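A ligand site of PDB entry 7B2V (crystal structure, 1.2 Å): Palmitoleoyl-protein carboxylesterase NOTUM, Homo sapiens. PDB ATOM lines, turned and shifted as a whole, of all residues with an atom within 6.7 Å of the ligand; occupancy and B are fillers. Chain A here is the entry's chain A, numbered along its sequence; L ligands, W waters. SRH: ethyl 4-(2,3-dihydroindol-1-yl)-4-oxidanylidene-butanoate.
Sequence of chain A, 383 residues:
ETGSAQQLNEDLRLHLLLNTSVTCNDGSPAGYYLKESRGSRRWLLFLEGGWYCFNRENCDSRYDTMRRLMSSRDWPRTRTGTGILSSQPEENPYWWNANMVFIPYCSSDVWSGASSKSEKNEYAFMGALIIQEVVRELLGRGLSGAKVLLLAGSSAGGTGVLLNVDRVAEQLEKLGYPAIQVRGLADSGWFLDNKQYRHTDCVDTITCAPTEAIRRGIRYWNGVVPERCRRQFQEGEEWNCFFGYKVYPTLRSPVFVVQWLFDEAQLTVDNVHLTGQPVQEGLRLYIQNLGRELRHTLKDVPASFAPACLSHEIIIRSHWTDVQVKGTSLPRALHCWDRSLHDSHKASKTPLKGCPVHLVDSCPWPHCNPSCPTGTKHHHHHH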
ATOM      1  N   GLU A  48      -6.496  21.678  -1.851  1.00  0.00           N
ATOM      2  CA  GLU A  48      -7.623  21.189  -2.621  1.00  0.00           C
ATOM      3  C   GLU A  48      -7.225  19.913  -3.358  1.00  0.00           C
ATOM      4  O   GLU A  48      -6.055  19.729  -3.746  1.00  0.00           O
ATOM      5  CB  GLU A  48      -8.017  22.272  -3.620  1.00  0.00           C
ATOM      6  CG  GLU A  48      -9.263  21.974  -4.422  1.00  0.00           C
ATOM      7  CD  GLU A  48      -9.590  23.018  -5.466  1.00  0.00           C
ATOM      8  OE1 GLU A  48      -8.715  23.742  -5.908  1.00  0.00           O
ATOM      9  OE2 GLU A  48     -10.803  23.106  -5.850  1.00  0.00           O
ATOM     10  N   GLY A  49      -8.225  19.066  -3.625  1.00  0.00           N
ATOM     11  CA  GLY A  49      -8.039  17.901  -4.452  1.00  0.00           C
ATOM     12  C   GLY A  49      -8.644  18.053  -5.843  1.00  0.00           C
ATOM     13  O   GLY A  49      -9.041  19.135  -6.270  1.00  0.00           O
ATOM     14  N   GLY A  50      -8.759  16.914  -6.517  1.00  0.00           N
ATOM     15  CA  GLY A  50      -9.357  16.829  -7.836  1.00  0.00           C
ATOM     16  C   GLY A  50      -8.602  15.952  -8.829  1.00  0.00           C
ATOM     17  O   GLY A  50      -8.361  16.419  -9.963  1.00  0.00           O
ATOM     18  N   TRP A  51      -8.276  14.715  -8.491  1.00  0.00           N
ATOM     19  CA  TRP A  51      -7.609  13.764  -9.399  1.00  0.00           C
ATOM     20  C   TRP A  51      -6.290  14.387  -9.868  1.00  0.00           C
ATOM     21  O   TRP A  51      -5.539  14.921  -9.018  1.00  0.00           O
ATOM     22  CB  TRP A  51      -8.552  13.318 -10.504  1.00  0.00           C
ATOM     23  CG  TRP A  51      -9.717  12.526  -9.953  1.00  0.00           C
ATOM     24  CD1 TRP A  51     -10.904  13.037  -9.571  1.00  0.00           C
ATOM     25  CD2 TRP A  51      -9.755  11.116  -9.740  1.00  0.00           C
ATOM     26  NE1 TRP A  51     -11.726  11.993  -9.131  1.00  0.00           N
ATOM     27  CE2 TRP A  51     -11.031  10.820  -9.195  1.00  0.00           C
ATOM     28  CE3 TRP A  51      -8.837  10.088  -9.928  1.00  0.00           C
ATOM     29  CZ2 TRP A  51     -11.441   9.513  -8.886  1.00  0.00           C
ATOM     30  CZ3 TRP A  51      -9.232   8.755  -9.574  1.00  0.00           C
ATOM     31  CH2 TRP A  51     -10.538   8.502  -9.075  1.00  0.00           C
ATOM     32  N   TYR A  52      -5.941  14.248 -11.148  1.00  0.00           N
ATOM     33  CA  TYR A  52      -4.604  14.504 -11.673  1.00  0.00           C
ATOM     34  C   TYR A  52      -4.715  14.269 -13.171  1.00  0.00           C
ATOM     35  O   TYR A  52      -5.728  13.755 -13.645  1.00  0.00           O
ATOM     36  CB  TYR A  52      -3.510  13.597 -11.057  1.00  0.00           C
ATOM     37  CG  TYR A  52      -3.910  12.148 -10.957  1.00  0.00           C
ATOM     38  CD1 TYR A  52      -3.824  11.301 -12.044  1.00  0.00           C
ATOM     39  CD2 TYR A  52      -4.425  11.642  -9.786  1.00  0.00           C
ATOM     40  CE1 TYR A  52      -4.229   9.980 -11.971  1.00  0.00           C
ATOM     41  CE2 TYR A  52      -4.789  10.305  -9.675  1.00  0.00           C
ATOM     42  CZ  TYR A  52      -4.724   9.487 -10.765  1.00  0.00           C
ATOM     43  OH  TYR A  52      -5.142   8.170 -10.618  1.00  0.00           O
ATOM     44  N   TYR A 105      -5.839  23.767  -6.109  1.00  0.00           N
ATOM     45  CA  TYR A 105      -5.081  22.727  -6.817  1.00  0.00           C
ATOM     46  C   TYR A 105      -5.125  23.049  -8.294  1.00  0.00           C
ATOM     47  O   TYR A 105      -6.131  22.856  -8.954  1.00  0.00           O
ATOM     48  CB  TYR A 105      -5.763  21.398  -6.527  1.00  0.00           C
ATOM     49  CG  TYR A 105      -5.157  20.183  -7.158  1.00  0.00           C
ATOM     50  CD1 TYR A 105      -3.773  19.967  -7.183  1.00  0.00           C
ATOM     51  CD2 TYR A 105      -5.986  19.155  -7.594  1.00  0.00           C
ATOM     52  CE1 TYR A 105      -3.253  18.754  -7.696  1.00  0.00           C
ATOM     53  CE2 TYR A 105      -5.472  17.974  -8.081  1.00  0.00           C
ATOM     54  CZ  TYR A 105      -4.125  17.782  -8.146  1.00  0.00           C
ATOM     55  OH  TYR A 105      -3.582  16.618  -8.611  1.00  0.00           O
ATOM     56  N   VAL A 110      -0.892  15.796  -8.000  1.00  0.00           N
ATOM     57  CA  VAL A 110      -1.055  15.281  -6.620  1.00  0.00           C
ATOM     58  C   VAL A 110      -0.077  16.101  -5.750  1.00  0.00           C
ATOM     59  O   VAL A 110       0.456  15.595  -4.757  1.00  0.00           O
ATOM     60  CB  VAL A 110      -0.794  13.754  -6.528  1.00  0.00           C
ATOM     61  CG1 VAL A 110      -1.261  13.216  -5.171  1.00  0.00           C
ATOM     62  CG2 VAL A 110      -1.433  13.007  -7.694  1.00  0.00           C
ATOM     63  N   SER A 154      -7.714  17.244   0.957  1.00  0.00           N
ATOM     64  CA  SER A 154      -8.699  16.204   0.656  1.00  0.00           C
ATOM     65  C   SER A 154      -8.435  15.585  -0.710  1.00  0.00           C
ATOM     66  O   SER A 154      -8.083  16.283  -1.666  1.00  0.00           O
ATOM     67  CB  SER A 154     -10.145  16.754   0.640  1.00  0.00           C
ATOM     68  OG  SER A 154     -10.496  17.229   1.929  1.00  0.00           O
ATOM     69  N   SER A 155      -8.640  14.260  -0.808  1.00  0.00           N
ATOM     70  CA  SER A 155      -8.461  13.482  -2.031  1.00  0.00           C
ATOM     71  C   SER A 155      -7.009  13.658  -2.487  1.00  0.00           C
ATOM     72  O   SER A 155      -6.102  13.347  -1.708  1.00  0.00           O
ATOM     73  CB  SER A 155      -9.565  13.790  -3.044  1.00  0.00           C
ATOM     74  OG  SER A 155      -9.551  12.749  -4.054  1.00  0.00           O
ATOM     75  N   ALA A 156      -6.736  14.094  -3.724  1.00  0.00           N
ATOM     76  CA  ALA A 156      -5.338  14.314  -4.138  1.00  0.00           C
ATOM     77  C   ALA A 156      -4.627  15.284  -3.180  1.00  0.00           C
ATOM     78  O   ALA A 156      -3.409  15.235  -3.036  1.00  0.00           O
ATOM     79  CB  ALA A 156      -5.265  14.840  -5.598  1.00  0.00           C
ATOM     80  N   GLY A 157      -5.391  16.227  -2.585  1.00  0.00           N
ATOM     81  CA  GLY A 157      -4.771  17.098  -1.589  1.00  0.00           C
ATOM     82  C   GLY A 157      -4.395  16.359  -0.309  1.00  0.00           C
ATOM     83  O   GLY A 157      -3.432  16.737   0.360  1.00  0.00           O
ATOM     84  N   THR A 159      -3.385  13.123  -0.256  1.00  0.00           N
ATOM     85  CA  THR A 159      -2.120  12.508  -0.629  1.00  0.00           C
ATOM     86  C   THR A 159      -1.015  13.571  -0.667  1.00  0.00           C
ATOM     87  O   THR A 159       0.100  13.333  -0.202  1.00  0.00           O
ATOM     88  CB  THR A 159      -2.263  11.793  -1.985  1.00  0.00           C
ATOM     89  OG1 THR A 159      -3.448  10.993  -1.990  1.00  0.00           O
ATOM     90  CG2 THR A 159      -1.010  10.939  -2.241  1.00  0.00           C
ATOM     91  N   SER A 188      -9.147  11.453   2.854  1.00  0.00           N
ATOM     92  CA  SER A 188      -9.517  10.799   1.599  1.00  0.00           C
ATOM     93  C   SER A 188      -8.347  10.739   0.643  1.00  0.00           C
ATOM     94  O   SER A 188      -8.566  10.742  -0.597  1.00  0.00           O
ATOM     95  CB  SER A 188     -10.714  11.479   0.979  1.00  0.00           C
ATOM     96  OG  SER A 188     -11.787  11.393   1.981  1.00  0.00           O
ATOM     97  N   GLY A 189      -7.126  10.647   1.139  1.00  0.00           N
ATOM     98  CA  GLY A 189      -5.926  10.502   0.311  1.00  0.00           C
ATOM     99  C   GLY A 189      -5.134   9.249   0.600  1.00  0.00           C
ATOM    100  O   GLY A 189      -3.956   9.188   0.225  1.00  0.00           O
ATOM    101  N   PHE A 191      -4.955   5.614  -0.264  1.00  0.00           N
ATOM    102  CA  PHE A 191      -5.425   4.660  -1.269  1.00  0.00           C
ATOM    103  C   PHE A 191      -4.633   3.382  -1.223  1.00  0.00           C
ATOM    104  O   PHE A 191      -3.499   3.348  -0.755  1.00  0.00           O
ATOM    105  CB  PHE A 191      -5.319   5.305  -2.657  1.00  0.00           C
ATOM    106  CG  PHE A 191      -6.179   6.536  -2.763  1.00  0.00           C
ATOM    107  CD1 PHE A 191      -7.540   6.401  -2.696  1.00  0.00           C
ATOM    108  CD2 PHE A 191      -5.632   7.810  -2.850  1.00  0.00           C
ATOM    109  CE1 PHE A 191      -8.378   7.513  -2.727  1.00  0.00           C
ATOM    110  CE2 PHE A 191      -6.470   8.926  -2.904  1.00  0.00           C
ATOM    111  CZ  PHE A 191      -7.801   8.794  -2.864  1.00  0.00           C
ATOM    112  N   PRO A 210      -4.111   3.413 -11.004  1.00  0.00           N
ATOM    113  CA  PRO A 210      -3.285   4.473 -10.388  1.00  0.00           C
ATOM    114  C   PRO A 210      -1.830   4.131 -10.252  1.00  0.00           C
ATOM    115  O   PRO A 210      -1.009   5.037 -10.444  1.00  0.00           O
ATOM    116  CB  PRO A 210      -3.946   4.673  -9.003  1.00  0.00           C
ATOM    117  CG  PRO A 210      -5.397   4.375  -9.310  1.00  0.00           C
ATOM    118  CD  PRO A 210      -5.366   3.202 -10.253  1.00  0.00           C
ATOM    119  N   THR A 211      -1.448   2.886  -9.984  1.00  0.00           N
ATOM    120  CA  THR A 211      -0.007   2.611  -9.944  1.00  0.00           C
ATOM    121  C   THR A 211       0.669   2.960 -11.255  1.00  0.00           C
ATOM    122  O   THR A 211       1.738   3.577 -11.230  1.00  0.00           O
ATOM    123  CB  THR A 211       0.313   1.184  -9.542  1.00  0.00           C
ATOM    124  OG1 THR A 211      -0.249   0.285 -10.480  1.00  0.00           O
ATOM    125  CG2 THR A 211      -0.205   0.857  -8.140  1.00  0.00           C
ATOM    126  N   ILE A 214       0.325   6.881 -11.963  1.00  0.00           N
ATOM    127  CA  ILE A 214       1.267   7.618 -11.120  1.00  0.00           C
ATOM    128  C   ILE A 214       2.717   7.394 -11.582  1.00  0.00           C
ATOM    129  O   ILE A 214       3.495   8.349 -11.620  1.00  0.00           O
ATOM    130  CB  ILE A 214       1.047   7.207  -9.649  1.00  0.00           C
ATOM    131  CG1 ILE A 214      -0.329   7.682  -9.142  1.00  0.00           C
ATOM    132  CG2 ILE A 214       2.156   7.785  -8.749  1.00  0.00           C
ATOM    133  CD1 ILE A 214      -0.547   9.167  -9.170  1.00  0.00           C
ATOM    134  N   PHE A 242       3.185   7.387  -3.202  1.00  0.00           N
ATOM    135  CA  PHE A 242       1.869   8.008  -3.299  1.00  0.00           C
ATOM    136  C   PHE A 242       0.811   7.200  -2.587  1.00  0.00           C
ATOM    137  O   PHE A 242      -0.348   7.621  -2.554  1.00  0.00           O
ATOM    138  CB  PHE A 242       1.509   8.170  -4.788  1.00  0.00           C
ATOM    139  CG  PHE A 242       2.204   9.326  -5.469  1.00  0.00           C
ATOM    140  CD1 PHE A 242       3.574   9.348  -5.648  1.00  0.00           C
ATOM    141  CD2 PHE A 242       1.460  10.364  -6.052  1.00  0.00           C
ATOM    142  CE1 PHE A 242       4.208  10.413  -6.340  1.00  0.00           C
ATOM    143  CE2 PHE A 242       2.118  11.404  -6.722  1.00  0.00           C
ATOM    144  CZ  PHE A 242       3.433  11.439  -6.852  1.00  0.00           C
ATOM    145  N   PHE A 243       1.181   6.052  -2.037  1.00  0.00           N
ATOM    146  CA  PHE A 243       0.241   5.169  -1.351  1.00  0.00           C
ATOM    147  C   PHE A 243       0.463   5.304   0.139  1.00  0.00           C
ATOM    148  O   PHE A 243       1.542   4.969   0.642  1.00  0.00           O
ATOM    149  CB  PHE A 243       0.375   3.728  -1.858  1.00  0.00           C
ATOM    150  CG  PHE A 243      -0.148   3.629  -3.240  1.00  0.00           C
ATOM    151  CD1 PHE A 243      -1.489   3.398  -3.477  1.00  0.00           C
ATOM    152  CD2 PHE A 243       0.656   3.948  -4.328  1.00  0.00           C
ATOM    153  CE1 PHE A 243      -2.002   3.433  -4.765  1.00  0.00           C
ATOM    154  CE2 PHE A 243       0.153   3.982  -5.607  1.00  0.00           C
ATOM    155  CZ  PHE A 243      -1.193   3.731  -5.808  1.00  0.00           C
ATOM    156  N   ASP A 263     -14.085   4.237   0.238  1.00  0.00           N
ATOM    157  CA  ASP A 263     -13.985   5.507  -0.454  1.00  0.00           C
ATOM    158  C   ASP A 263     -14.433   5.368  -1.913  1.00  0.00           C
ATOM    159  O   ASP A 263     -14.024   4.429  -2.622  1.00  0.00           O
ATOM    160  CB  ASP A 263     -12.552   5.993  -0.362  1.00  0.00           C
ATOM    161  CG  ASP A 263     -12.380   7.329  -0.926  1.00  0.00           C
ATOM    162  OD1 ASP A 263     -12.561   8.326  -0.250  1.00  0.00           O
ATOM    163  OD2 ASP A 263     -12.047   7.398  -2.124  1.00  0.00           O
ATOM    164  N   ALA A 265     -13.678   7.076  -4.556  1.00  0.00           N
ATOM    165  CA  ALA A 265     -12.582   7.129  -5.525  1.00  0.00           C
ATOM    166  C   ALA A 265     -11.791   5.835  -5.538  1.00  0.00           C
ATOM    167  O   ALA A 265     -11.327   5.402  -6.607  1.00  0.00           O
ATOM    168  CB  ALA A 265     -11.702   8.341  -5.232  1.00  0.00           C
ATOM    169  N   GLN A 266     -11.576   5.203  -4.367  1.00  0.00           N
ATOM    170  CA  GLN A 266     -10.947   3.878  -4.354  1.00  0.00           C
ATOM    171  C   GLN A 266     -11.775   2.878  -5.150  1.00  0.00           C
ATOM    172  O   GLN A 266     -11.252   2.144  -5.997  1.00  0.00           O
ATOM    173  CB  GLN A 266     -10.800   3.417  -2.917  1.00  0.00           C
ATOM    174  CG  GLN A 266     -10.194   2.035  -2.784  1.00  0.00           C
ATOM    175  CD  GLN A 266      -8.699   2.028  -3.011  1.00  0.00           C
ATOM    176  OE1 GLN A 266      -7.988   2.838  -2.413  1.00  0.00           O
ATOM    177  NE2 GLN A 266      -8.218   1.145  -3.890  1.00  0.00           N
ATOM    178  N   VAL A 269     -11.287   3.500  -8.951  1.00  0.00           N
ATOM    179  CA  VAL A 269     -10.031   2.981  -9.499  1.00  0.00           C
ATOM    180  C   VAL A 269      -9.951   1.464  -9.419  1.00  0.00           C
ATOM    181  O   VAL A 269      -9.150   0.850 -10.135  1.00  0.00           O
ATOM    182  CB  VAL A 269      -8.779   3.657  -8.917  1.00  0.00           C
ATOM    183  CG1 VAL A 269      -8.838   5.158  -9.175  1.00  0.00           C
ATOM    184  CG2 VAL A 269      -8.613   3.338  -7.421  1.00  0.00           C
ATOM    185  N   HIS A 312     -16.806  10.179   0.064  1.00  0.00           N
ATOM    186  CA  HIS A 312     -15.553  10.702  -0.453  1.00  0.00           C
ATOM    187  C   HIS A 312     -15.361  12.113   0.075  1.00  0.00           C
ATOM    188  O   HIS A 312     -16.203  12.977  -0.203  1.00  0.00           O
ATOM    189  CB  HIS A 312     -15.589  10.739  -1.983  1.00  0.00           C
ATOM    190  CG  HIS A 312     -14.303  11.179  -2.592  1.00  0.00           C
ATOM    191  ND1 HIS A 312     -13.095  10.553  -2.350  1.00  0.00           N
ATOM    192  CD2 HIS A 312     -14.041  12.193  -3.456  1.00  0.00           C
ATOM    193  CE1 HIS A 312     -12.146  11.168  -3.030  1.00  0.00           C
ATOM    194  NE2 HIS A 312     -12.691  12.156  -3.711  1.00  0.00           N
ATOM    195  N   GLU A 313     -14.243  12.337   0.760  1.00  0.00           N
ATOM    196  CA  GLU A 313     -13.831  13.593   1.428  1.00  0.00           C
ATOM    197  C   GLU A 313     -14.749  13.874   2.602  1.00  0.00           C
ATOM    198  O   GLU A 313     -15.853  13.333   2.681  1.00  0.00           O
ATOM    199  CB  GLU A 313     -13.799  14.780   0.474  1.00  0.00           C
ATOM    200  CG  GLU A 313     -12.929  14.530  -0.771  1.00  0.00           C
ATOM    201  CD  GLU A 313     -12.864  15.707  -1.676  1.00  0.00           C
ATOM    202  OE1 GLU A 313     -11.751  16.011  -2.141  1.00  0.00           O
ATOM    203  OE2 GLU A 313     -13.930  16.295  -1.977  1.00  0.00           O
HETATM  204  C04 SRH L   1      -9.375  13.073  -5.384  1.00  0.00           C
HETATM  205  C06 SRH L   1      -9.699  11.969  -6.371  1.00  0.00           C
HETATM  206  C07 SRH L   1      -9.065  10.621  -6.085  1.00  0.00           C
HETATM  207  C08 SRH L   1      -7.556  10.653  -6.083  1.00  0.00           C
HETATM  208  C11 SRH L   1      -7.496   8.158  -6.345  1.00  0.00           C
HETATM  209  C12 SRH L   1      -6.405   7.158  -6.550  1.00  0.00           C
HETATM  210  C13 SRH L   1      -5.131   7.909  -6.175  1.00  0.00           C
HETATM  211  C14 SRH L   1      -3.842   7.409  -5.964  1.00  0.00           C
HETATM  212  C15 SRH L   1      -2.854   8.332  -5.566  1.00  0.00           C
HETATM  213  C16 SRH L   1      -3.158   9.711  -5.461  1.00  0.00           C
HETATM  214  C17 SRH L   1      -4.439  10.200  -5.661  1.00  0.00           C
HETATM  215  C18 SRH L   1      -5.408   9.277  -6.073  1.00  0.00           C
HETATM  216  N10 SRH L   1      -6.837   9.448  -6.228  1.00  0.00           N
HETATM  217  O05 SRH L   1      -8.879  14.093  -5.729  1.00  0.00           O
HETATM  218  O09 SRH L   1      -6.940  11.671  -5.929  1.00  0.00           O
HETATM  219  O   HOH W   1     -11.973  14.153  -5.559  1.00  0.00           O
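Water W1 lies within hydrogen-bond range of NE2 of His 312, O05 of the ligand and OG of Ser 155.
OG of Ser 155 is covalently linked to C04 of the ligand, 1.4 Å away. The backbone NH of Trp 51 lies within hydrogen-bond range of an oxygen (O05) of the ligand (2.9 Å). O05 of the ligand lies within hydrogen-bond range of N of Gly 50, 2.9 Å away. N of Ala 156 is in hydrogen-bond range of O05 of the ligand.
Gly 49 touches the ligand. Tyr 52 touches the ligand. CG1 of Val 110 touches C16 of the ligand, 3.996 Å away. Thr 159 touches the ligand. CE2 of Phe 191 touches C18 of the ligand, 3.4 Å away. Phe 242 touches the ligand. Ala 265 touches the ligand. His 312 touches the ligand (NE2 to C04, 3.8 Å). Hydrophobic or aromatic side chains within 4 Å of the ligand: Trp 51, Tyr 52, Val 110, Ala 156, Phe 191 and Ala 265. 12 residues have an atom within 4 Å of the ligand: Gly 49, Gly 50, Trp 51, Tyr 52, Val 110, Ser 155, Ala 156, Thr 159, Phe 191, Phe 242, Ala 265 and His 312. Along chain A the residues within 4 Å of the ligand span positions 49 to 312. The nearest printed residue that does not touch the ligand is Pro 210 (4.05 Å).
The side-chain hydroxyl of Ser 155 sits close to a ring nitrogen (NE2) of His 312 (3.2 Å). The backbone carbonyl oxygen of Trp 51 lies within hydrogen-bond range of the side-chain hydroxyl of Tyr 105, 2.6 Å away. The backbone NH (N) of Ala 265 lies within hydrogen-bond range of the side-chain carboxylate (OD2) of Asp 263, 2.9 Å away. O of Gly 189 is in hydrogen-bond range of OG1 of Thr 159. A ring nitrogen (ND1) of His 312 sits at hydrogen-bond distance from the side-chain carboxylate (OD1) of Asp 263 (3.1 Å). The backbone NH (N) of Gly 49 lies close to the backbone carbonyl oxygen (O) of Ser 154, at 3.4 Å. The backbone NH of Val 110 sits at hydrogen-bond distance from the side-chain hydroxyl of Tyr 105 (2.9 Å).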
